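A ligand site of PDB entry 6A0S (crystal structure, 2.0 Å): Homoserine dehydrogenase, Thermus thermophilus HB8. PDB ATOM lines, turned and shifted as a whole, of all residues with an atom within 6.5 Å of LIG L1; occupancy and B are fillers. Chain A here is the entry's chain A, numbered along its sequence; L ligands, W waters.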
ATOM      1  N   ALA A  97      14.969 -21.684  19.428  1.00  0.00           N
ATOM      2  CA  ALA A  97      15.733 -20.844  20.322  1.00  0.00           C
ATOM      3  C   ALA A  97      14.938 -20.446  21.563  1.00  0.00           C
ATOM      4  O   ALA A  97      15.395 -19.656  22.371  1.00  0.00           O
ATOM      5  CB  ALA A  97      16.233 -19.629  19.615  1.00  0.00           C
ATOM      6  N   LYS A  99      13.869 -20.685  24.965  1.00  0.00           N
ATOM      7  CA  LYS A  99      14.228 -21.180  26.263  1.00  0.00           C
ATOM      8  C   LYS A  99      13.057 -21.221  27.210  1.00  0.00           C
ATOM      9  O   LYS A  99      12.960 -22.145  28.046  1.00  0.00           O
ATOM     10  CB  LYS A  99      15.363 -20.382  26.880  1.00  0.00           C
ATOM     11  CG  LYS A  99      15.036 -18.964  27.289  1.00  0.00           C
ATOM     12  CD  LYS A  99      14.679 -18.060  26.177  1.00  0.00           C
ATOM     13  CE  LYS A  99      15.801 -17.559  25.358  1.00  0.00           C
ATOM     14  NZ  LYS A  99      15.759 -16.068  25.265  1.00  0.00           N
ATOM     15  N   ALA A 122      20.545 -22.854  20.093  1.00  0.00           N
ATOM     16  CA  ALA A 122      20.357 -21.371  20.128  1.00  0.00           C
ATOM     17  C   ALA A 122      19.540 -20.901  21.348  1.00  0.00           C
ATOM     18  O   ALA A 122      19.516 -19.688  21.619  1.00  0.00           O
ATOM     19  CB  ALA A 122      19.695 -20.856  18.845  1.00  0.00           C
ATOM     20  N   SER A 123      18.949 -21.815  22.088  1.00  0.00           N
ATOM     21  CA  SER A 123      18.214 -21.483  23.377  1.00  0.00           C
ATOM     22  C   SER A 123      19.094 -21.041  24.574  1.00  0.00           C
ATOM     23  O   SER A 123      18.625 -20.436  25.573  1.00  0.00           O
ATOM     24  CB  SER A 123      17.344 -22.616  23.753  1.00  0.00           C
ATOM     25  OG  SER A 123      17.990 -23.742  24.291  1.00  0.00           O
ATOM     26  N   VAL A 124      20.406 -21.295  24.483  1.00  0.00           N
ATOM     27  CA  VAL A 124      21.303 -20.819  25.552  1.00  0.00           C
ATOM     28  C   VAL A 124      22.572 -20.341  24.929  1.00  0.00           C
ATOM     29  O   VAL A 124      23.302 -21.065  24.208  1.00  0.00           O
ATOM     30  CB  VAL A 124      21.653 -22.001  26.526  1.00  0.00           C
ATOM     31  CG1 VAL A 124      22.665 -21.538  27.551  1.00  0.00           C
ATOM     32  CG2 VAL A 124      20.417 -22.576  27.138  1.00  0.00           C
ATOM     33  N   MET A 125      22.853 -19.090  25.208  1.00  0.00           N
ATOM     34  CA  MET A 125      23.961 -18.379  24.665  1.00  0.00           C
ATOM     35  C   MET A 125      23.932 -18.353  23.149  1.00  0.00           C
ATOM     36  O   MET A 125      25.011 -18.286  22.491  1.00  0.00           O
ATOM     37  CB  MET A 125      25.342 -18.894  25.206  1.00  0.00           C
ATOM     38  CG  MET A 125      25.383 -18.682  26.692  1.00  0.00           C
ATOM     39  SD  MET A 125      26.825 -19.389  27.544  1.00  0.00           S
ATOM     40  CE  MET A 125      28.164 -18.945  26.553  1.00  0.00           C
ATOM     41  N   ALA A 126      22.738 -18.289  22.596  1.00  0.00           N
ATOM     42  CA  ALA A 126      22.601 -18.128  21.152  1.00  0.00           C
ATOM     43  C   ALA A 126      23.476 -19.132  20.374  1.00  0.00           C
ATOM     44  O   ALA A 126      23.573 -20.231  20.794  1.00  0.00           O
ATOM     45  CB  ALA A 126      22.877 -16.694  20.798  1.00  0.00           C
ATOM     46  N   LEU A 149      24.530 -16.056  31.731  1.00  0.00           N
ATOM     47  CA  LEU A 149      23.666 -16.536  30.638  1.00  0.00           C
ATOM     48  C   LEU A 149      22.694 -15.513  30.043  1.00  0.00           C
ATOM     49  O   LEU A 149      22.156 -15.755  29.004  1.00  0.00           O
ATOM     50  CB  LEU A 149      22.885 -17.729  31.070  1.00  0.00           C
ATOM     51  CG  LEU A 149      23.684 -18.866  31.776  1.00  0.00           C
ATOM     52  CD1 LEU A 149      22.705 -19.953  32.159  1.00  0.00           C
ATOM     53  CD2 LEU A 149      24.719 -19.464  30.766  1.00  0.00           C
ATOM     54  N   ASN A 150      22.669 -14.312  30.585  1.00  0.00           N
ATOM     55  CA  ASN A 150      21.674 -13.310  30.089  1.00  0.00           C
ATOM     56  C   ASN A 150      22.476 -12.213  29.494  1.00  0.00           C
ATOM     57  O   ASN A 150      23.168 -11.452  30.158  1.00  0.00           O
ATOM     58  CB  ASN A 150      20.683 -12.857  31.234  1.00  0.00           C
ATOM     59  CG  ASN A 150      19.641 -11.859  30.712  1.00  0.00           C
ATOM     60  OD1 ASN A 150      19.886 -10.725  30.775  1.00  0.00           O
ATOM     61  ND2 ASN A 150      18.750 -12.354  29.937  1.00  0.00           N
ATOM     62  N   GLY A 151      22.340 -12.094  28.188  1.00  0.00           N
ATOM     63  CA  GLY A 151      23.029 -11.044  27.477  1.00  0.00           C
ATOM     64  C   GLY A 151      22.603  -9.640  27.870  1.00  0.00           C
ATOM     65  O   GLY A 151      23.412  -8.771  28.111  1.00  0.00           O
ATOM     66  N   THR A 152      21.275  -9.411  27.990  1.00  0.00           N
ATOM     67  CA  THR A 152      20.817  -8.085  28.334  1.00  0.00           C
ATOM     68  C   THR A 152      21.373  -7.615  29.645  1.00  0.00           C
ATOM     69  O   THR A 152      21.815  -6.473  29.764  1.00  0.00           O
ATOM     70  CB  THR A 152      19.245  -8.131  28.368  1.00  0.00           C
ATOM     71  OG1 THR A 152      18.794  -8.441  27.044  1.00  0.00           O
ATOM     72  CG2 THR A 152      18.705  -6.900  28.924  1.00  0.00           C
ATOM     73  N   THR A 153      21.308  -8.420  30.727  1.00  0.00           N
ATOM     74  CA  THR A 153      21.800  -7.918  32.000  1.00  0.00           C
ATOM     75  C   THR A 153      23.360  -7.805  32.117  1.00  0.00           C
ATOM     76  O   THR A 153      23.918  -7.077  32.968  1.00  0.00           O
ATOM     77  CB  THR A 153      21.304  -8.734  33.221  1.00  0.00           C
ATOM     78  OG1 THR A 153      21.433 -10.135  33.046  1.00  0.00           O
ATOM     79  CG2 THR A 153      19.728  -8.576  33.341  1.00  0.00           C
ATOM     80  N   GLY A 177      18.459  -5.358  20.132  1.00  0.00           N
ATOM     81  CA  GLY A 177      17.651  -6.545  19.919  1.00  0.00           C
ATOM     82  C   GLY A 177      18.006  -7.647  20.910  1.00  0.00           C
ATOM     83  O   GLY A 177      17.667  -8.797  20.681  1.00  0.00           O
ATOM     84  N   TYR A 178      18.721  -7.305  21.975  1.00  0.00           N
ATOM     85  CA  TYR A 178      19.074  -8.333  23.032  1.00  0.00           C
ATOM     86  C   TYR A 178      17.936  -8.725  23.984  1.00  0.00           C
ATOM     87  O   TYR A 178      17.882  -9.886  24.350  1.00  0.00           O
ATOM     88  CB  TYR A 178      20.189  -7.787  23.920  1.00  0.00           C
ATOM     89  CG  TYR A 178      21.475  -7.500  23.197  1.00  0.00           C
ATOM     90  CD1 TYR A 178      21.770  -8.029  21.911  1.00  0.00           C
ATOM     91  CD2 TYR A 178      22.408  -6.706  23.813  1.00  0.00           C
ATOM     92  CE1 TYR A 178      22.977  -7.716  21.278  1.00  0.00           C
ATOM     93  CE2 TYR A 178      23.595  -6.376  23.191  1.00  0.00           C
ATOM     94  CZ  TYR A 178      23.902  -6.909  21.970  1.00  0.00           C
ATOM     95  OH  TYR A 178      25.097  -6.581  21.456  1.00  0.00           O
ATOM     96  N   ALA A 179      17.057  -7.771  24.395  1.00  0.00           N
ATOM     97  CA  ALA A 179      15.991  -8.008  25.444  1.00  0.00           C
ATOM     98  C   ALA A 179      14.867  -8.872  25.040  1.00  0.00           C
ATOM     99  O   ALA A 179      14.489  -8.952  23.864  1.00  0.00           O
ATOM    100  CB  ALA A 179      15.502  -6.721  26.045  1.00  0.00           C
ATOM    101  N   GLU A 180      14.373  -9.684  25.984  1.00  0.00           N
ATOM    102  CA  GLU A 180      13.129 -10.355  25.796  1.00  0.00           C
ATOM    103  C   GLU A 180      12.022  -9.219  25.585  1.00  0.00           C
ATOM    104  O   GLU A 180      12.164  -8.067  26.035  1.00  0.00           O
ATOM    105  CB  GLU A 180      12.759 -11.202  27.040  1.00  0.00           C
ATOM    106  CG  GLU A 180      13.646 -12.448  27.235  1.00  0.00           C
ATOM    107  CD  GLU A 180      13.736 -13.173  25.926  1.00  0.00           C
ATOM    108  OE1 GLU A 180      14.807 -13.153  25.305  1.00  0.00           O
ATOM    109  OE2 GLU A 180      12.702 -13.667  25.435  1.00  0.00           O
ATOM    110  N   ASP A 186      14.628 -10.675  31.603  1.00  0.00           N
ATOM    111  CA  ASP A 186      16.024 -10.430  31.658  1.00  0.00           C
ATOM    112  C   ASP A 186      16.438  -9.932  32.994  1.00  0.00           C
ATOM    113  O   ASP A 186      17.342 -10.507  33.608  1.00  0.00           O
ATOM    114  CB  ASP A 186      16.490  -9.448  30.550  1.00  0.00           C
ATOM    115  CG  ASP A 186      16.121  -9.886  29.222  1.00  0.00           C
ATOM    116  OD1 ASP A 186      16.567 -11.021  28.841  1.00  0.00           O
ATOM    117  OD2 ASP A 186      15.397  -9.127  28.479  1.00  0.00           O
ATOM    118  N   ASP A 191      14.995 -15.271  32.692  1.00  0.00           N
ATOM    119  CA  ASP A 191      15.577 -15.770  31.470  1.00  0.00           C
ATOM    120  C   ASP A 191      16.876 -16.633  31.782  1.00  0.00           C
ATOM    121  O   ASP A 191      16.975 -17.705  31.218  1.00  0.00           O
ATOM    122  CB  ASP A 191      15.891 -14.596  30.503  1.00  0.00           C
ATOM    123  CG  ASP A 191      16.633 -15.056  29.239  1.00  0.00           C
ATOM    124  OD1 ASP A 191      17.851 -14.833  29.255  1.00  0.00           O
ATOM    125  OD2 ASP A 191      16.019 -15.652  28.358  1.00  0.00           O
ATOM    126  N   LYS A 195      17.320 -20.774  31.173  1.00  0.00           N
ATOM    127  CA  LYS A 195      18.567 -21.324  30.553  1.00  0.00           C
ATOM    128  C   LYS A 195      19.248 -22.286  31.526  1.00  0.00           C
ATOM    129  O   LYS A 195      19.630 -23.388  31.122  1.00  0.00           O
ATOM    130  CB  LYS A 195      19.438 -20.163  30.189  1.00  0.00           C
ATOM    131  CG  LYS A 195      18.826 -19.457  28.963  1.00  0.00           C
ATOM    132  CD  LYS A 195      19.492 -18.148  28.639  1.00  0.00           C
ATOM    133  CE  LYS A 195      18.894 -17.438  27.378  1.00  0.00           C
ATOM    134  NZ  LYS A 195      19.530 -16.118  27.420  1.00  0.00           N
ATOM    135  N   ASN A 270      28.581 -13.547  26.962  1.00  0.00           N
ATOM    136  CA  ASN A 270      28.156 -14.559  27.863  1.00  0.00           C
ATOM    137  C   ASN A 270      29.183 -15.688  28.065  1.00  0.00           C
ATOM    138  O   ASN A 270      30.038 -15.784  27.222  1.00  0.00           O
ATOM    139  CB  ASN A 270      26.886 -15.074  27.391  1.00  0.00           C
ATOM    140  CG  ASN A 270      25.771 -13.877  27.474  1.00  0.00           C
ATOM    141  OD1 ASN A 270      25.632 -13.116  26.559  1.00  0.00           O
ATOM    142  ND2 ASN A 270      25.371 -13.574  28.637  1.00  0.00           N
ATOM    143  N   GLY A 288      25.717 -13.963  23.418  1.00  0.00           N
ATOM    144  CA  GLY A 288      24.589 -14.716  23.933  1.00  0.00           C
ATOM    145  C   GLY A 288      23.211 -14.200  23.543  1.00  0.00           C
ATOM    146  O   GLY A 288      22.227 -14.757  23.989  1.00  0.00           O
ATOM    147  N   ALA A 289      23.188 -13.220  22.654  1.00  0.00           N
ATOM    148  CA  ALA A 289      21.952 -12.565  22.170  1.00  0.00           C
ATOM    149  C   ALA A 289      22.235 -11.915  20.844  1.00  0.00           C
ATOM    150  O   ALA A 289      23.436 -11.685  20.472  1.00  0.00           O
ATOM    151  CB  ALA A 289      21.518 -11.500  23.191  1.00  0.00           C
ATOM    152  N   GLY A 290      21.141 -11.592  20.120  1.00  0.00           N
ATOM    153  CA  GLY A 290      21.256 -10.861  18.820  1.00  0.00           C
ATOM    154  C   GLY A 290      20.701 -11.745  17.738  1.00  0.00           C
ATOM    155  O   GLY A 290      20.658 -12.999  17.862  1.00  0.00           O
ATOM    156  N   THR A 294      21.933 -15.657  17.111  1.00  0.00           N
ATOM    157  CA  THR A 294      20.943 -16.655  17.301  1.00  0.00           C
ATOM    158  C   THR A 294      20.704 -17.483  16.057  1.00  0.00           C
ATOM    159  O   THR A 294      20.617 -18.722  16.132  1.00  0.00           O
ATOM    160  CB  THR A 294      19.684 -16.079  17.861  1.00  0.00           C
ATOM    161  OG1 THR A 294      20.032 -15.310  18.993  1.00  0.00           O
ATOM    162  CG2 THR A 294      18.705 -17.050  18.157  1.00  0.00           C
HETATM  163  N1  LIG L   1      17.036 -11.606  26.245  1.00  0.00           N
HETATM  164  C1  LIG L   1      17.982 -12.742  26.089  1.00  0.00           C
HETATM  165  C2  LIG L   1      19.310 -12.339  26.689  1.00  0.00           C
HETATM  166  C3  LIG L   1      18.015 -13.281  24.611  1.00  0.00           C
HETATM  167  O1  LIG L   1      19.554 -11.188  27.035  1.00  0.00           O
HETATM  168  O2  LIG L   1      20.161 -13.238  26.913  1.00  0.00           O
HETATM  169  C4  LIG L   1      19.149 -14.376  24.338  1.00  0.00           C
HETATM  170  O3  LIG L   1      18.705 -15.669  24.678  1.00  0.00           O
HETATM  171  P1  LG2 L   2      10.637 -10.872  17.723  1.00  0.00           P
HETATM  172  O1  LG2 L   2       9.389 -10.399  18.476  1.00  0.00           O
HETATM  173  O2  LG2 L   2      11.643  -9.962  17.148  1.00  0.00           O
HETATM  174  O3  LG2 L   2       9.958 -11.840  16.704  1.00  0.00           O
HETATM  175  C1  LG2 L   2       8.781 -12.490  17.099  1.00  0.00           C
HETATM  176  C2  LG2 L   2       8.288 -12.982  15.754  1.00  0.00           C
HETATM  177  O4  LG2 L   2       7.249 -13.900  15.898  1.00  0.00           O
HETATM  178  C3  LG2 L   2       7.704 -11.817  14.870  1.00  0.00           C
HETATM  179  O5  LG2 L   2       7.961 -11.965  13.468  1.00  0.00           O
HETATM  180  C4  LG2 L   2       6.217 -11.855  15.048  1.00  0.00           C
HETATM  181  O6  LG2 L   2       5.407 -11.402  13.954  1.00  0.00           O
HETATM  182  C5  LG2 L   2       6.038 -13.339  15.309  1.00  0.00           C
HETATM  183  N1  LG2 L   2       5.089 -13.569  16.399  1.00  0.00           N
HETATM  184  C6  LG2 L   2       5.200 -13.140  17.686  1.00  0.00           C
HETATM  185  N2  LG2 L   2       4.191 -13.621  18.409  1.00  0.00           N
HETATM  186  C7  LG2 L   2       3.413 -14.383  17.607  1.00  0.00           C
HETATM  187  C8  LG2 L   2       2.138 -15.154  17.715  1.00  0.00           C
HETATM  188  N3  LG2 L   2       1.479 -15.320  18.875  1.00  0.00           N
HETATM  189  N4  LG2 L   2       1.696 -15.785  16.621  1.00  0.00           N
HETATM  190  C9  LG2 L   2       2.371 -15.715  15.434  1.00  0.00           C
HETATM  191  N5  LG2 L   2       3.513 -14.995  15.215  1.00  0.00           N
HETATM  192  C10 LG2 L   2       4.060 -14.369  16.272  1.00  0.00           C
HETATM  193  O7  LG2 L   2      11.388 -11.886  18.757  1.00  0.00           O
HETATM  194  P2  LG2 L   2      12.957 -12.361  18.559  1.00  0.00           P
HETATM  195  O8  LG2 L   2      12.910 -12.749  17.090  1.00  0.00           O
HETATM  196  O9  LG2 L   2      13.924 -11.484  19.294  1.00  0.00           O
HETATM  197  O10 LG2 L   2      12.787 -13.759  19.434  1.00  0.00           O
HETATM  198  C11 LG2 L   2      12.134 -14.881  18.971  1.00  0.00           C
HETATM  199  C12 LG2 L   2      12.553 -16.037  19.886  1.00  0.00           C
HETATM  200  O11 LG2 L   2      13.983 -16.218  19.881  1.00  0.00           O
HETATM  201  C13 LG2 L   2      12.141 -15.730  21.346  1.00  0.00           C
HETATM  202  O12 LG2 L   2      11.755 -16.966  22.002  1.00  0.00           O
HETATM  203  C14 LG2 L   2      13.363 -15.142  22.022  1.00  0.00           C
HETATM  204  O13 LG2 L   2      13.423 -15.463  23.405  1.00  0.00           O
HETATM  205  C15 LG2 L   2      14.407 -16.023  21.275  1.00  0.00           C
HETATM  206  N6  LG2 L   2      15.709 -15.510  21.280  1.00  0.00           N
HETATM  207  C16 LG2 L   2      15.921 -14.198  21.049  1.00  0.00           C
HETATM  208  C17 LG2 L   2      17.222 -13.712  20.963  1.00  0.00           C
HETATM  209  C18 LG2 L   2      17.523 -12.309  20.721  1.00  0.00           C
HETATM  210  O14 LG2 L   2      18.608 -11.961  21.106  1.00  0.00           O
HETATM  211  N7  LG2 L   2      16.609 -11.479  20.195  1.00  0.00           N
HETATM  212  C19 LG2 L   2      18.392 -14.629  21.123  1.00  0.00           C
HETATM  213  C20 LG2 L   2      18.059 -15.998  21.402  1.00  0.00           C
HETATM  214  C21 LG2 L   2      16.730 -16.393  21.443  1.00  0.00           C
HETATM  215  P3  LG2 L   2       5.605  -9.804  13.609  1.00  0.00           P
HETATM  216  O15 LG2 L   2       4.470  -9.539  12.585  1.00  0.00           O
HETATM  217  O16 LG2 L   2       5.526  -8.928  14.838  1.00  0.00           O
HETATM  218  O17 LG2 L   2       7.077  -9.522  13.199  1.00  0.00           O
HETATM  219  O   HOH W   1      19.950 -17.927  23.669  1.00  0.00           O
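The backbone NH (N) of Gly 288 lies close to the side-chain amide oxygen (OD1) of Asn 270.
O of Tyr 178 lies within hydrogen-bond range of OG1 of Thr 152 (3.2 Å).
OD1 of Asn 150 sits at hydrogen-bond distance from N of Thr 152, at 3.4 Å.
NZ of Lys 195 is in salt-bridge range of OD1 of Asp 191, at 2.8 Å.
The backbone NH (N) of Thr 153 is in hydrogen-bond range of the side-chain amide oxygen (OD1) of Asn 150.
The backbone NH (N) of Asn 150 sits close to the side-chain amide nitrogen (ND2) of Asn 270 (3.4 Å).
N of Gly 151 sits close to ND2 of Asn 270, at 3.4 Å.
The side-chain carboxylate (OD1) of Asp 186 is in hydrogen-bond range of the side-chain amide nitrogen (ND2) of Asn 150 (2.8 Å).
Residues that only touch LIG L1: Gly 288, Asp 191, Ala 179, Leu 149 and Ala 289.
Hydrophobic or aromatic side chains within 4 Å of LIG L1: Ala 289.
13 residues have an atom within 4 Å of LIG L1: Lys 99, Leu 149, Asn 150, Gly 151, Thr 152, Tyr 178, Ala 179, Glu 180, Asp 186, Asp 191, Lys 195, Gly 288 and Ala 289.
OD1 of Asp 186 lies within salt-bridge range of N1 of LIG L1 (2.7 Å).
The backbone NH of Glu 180 lies close to a nitrogen (N1) of LIG L1 (3.3 Å).
The backbone carbonyl oxygen (O) of Tyr 178 sits at hydrogen-bond distance from a nitrogen (N1) of LIG L1, at 2.7 Å.
N of Thr 152 sits at hydrogen-bond distance from O1 of LIG L1 (2.7 Å).
OE1 of Glu 180 is in salt-bridge range of N1 of LIG L1 (2.9 Å).
OE2 of Glu 180 lies within hydrogen-bond range of O13 of LG2 L2 (2.8 Å).
A nitrogen (N7) of LG2 L2 sits at hydrogen-bond distance from the backbone carbonyl oxygen of Gly 177 (2.9 Å).
The side-chain amino group (NZ) of Lys 99 is in hydrogen-bond range of an oxygen (O3) of LIG L1, 3.0 Å away.
The side-chain amide nitrogen (ND2) of Asn 150 is in hydrogen-bond range of an oxygen (O1) of LIG L1 (3.2 Å).
O13 of LG2 L2 lies within hydrogen-bond range of NZ of Lys 99 (3.0 Å).
An oxygen (O2) of LIG L1 lies within hydrogen-bond range of the backbone NH of Gly 151, 2.8 Å away.
The backbone NH of Gly 290 sits at hydrogen-bond distance from an oxygen (O14) of LG2 L2, 2.7 Å away.
O1 of LIG L1 lies within hydrogen-bond range of OG1 of Thr 152, 2.9 Å away.
The side-chain amino group (NZ) of Lys 195 is in salt-bridge range of an oxygen (O2) of LIG L1 (3.0 Å).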
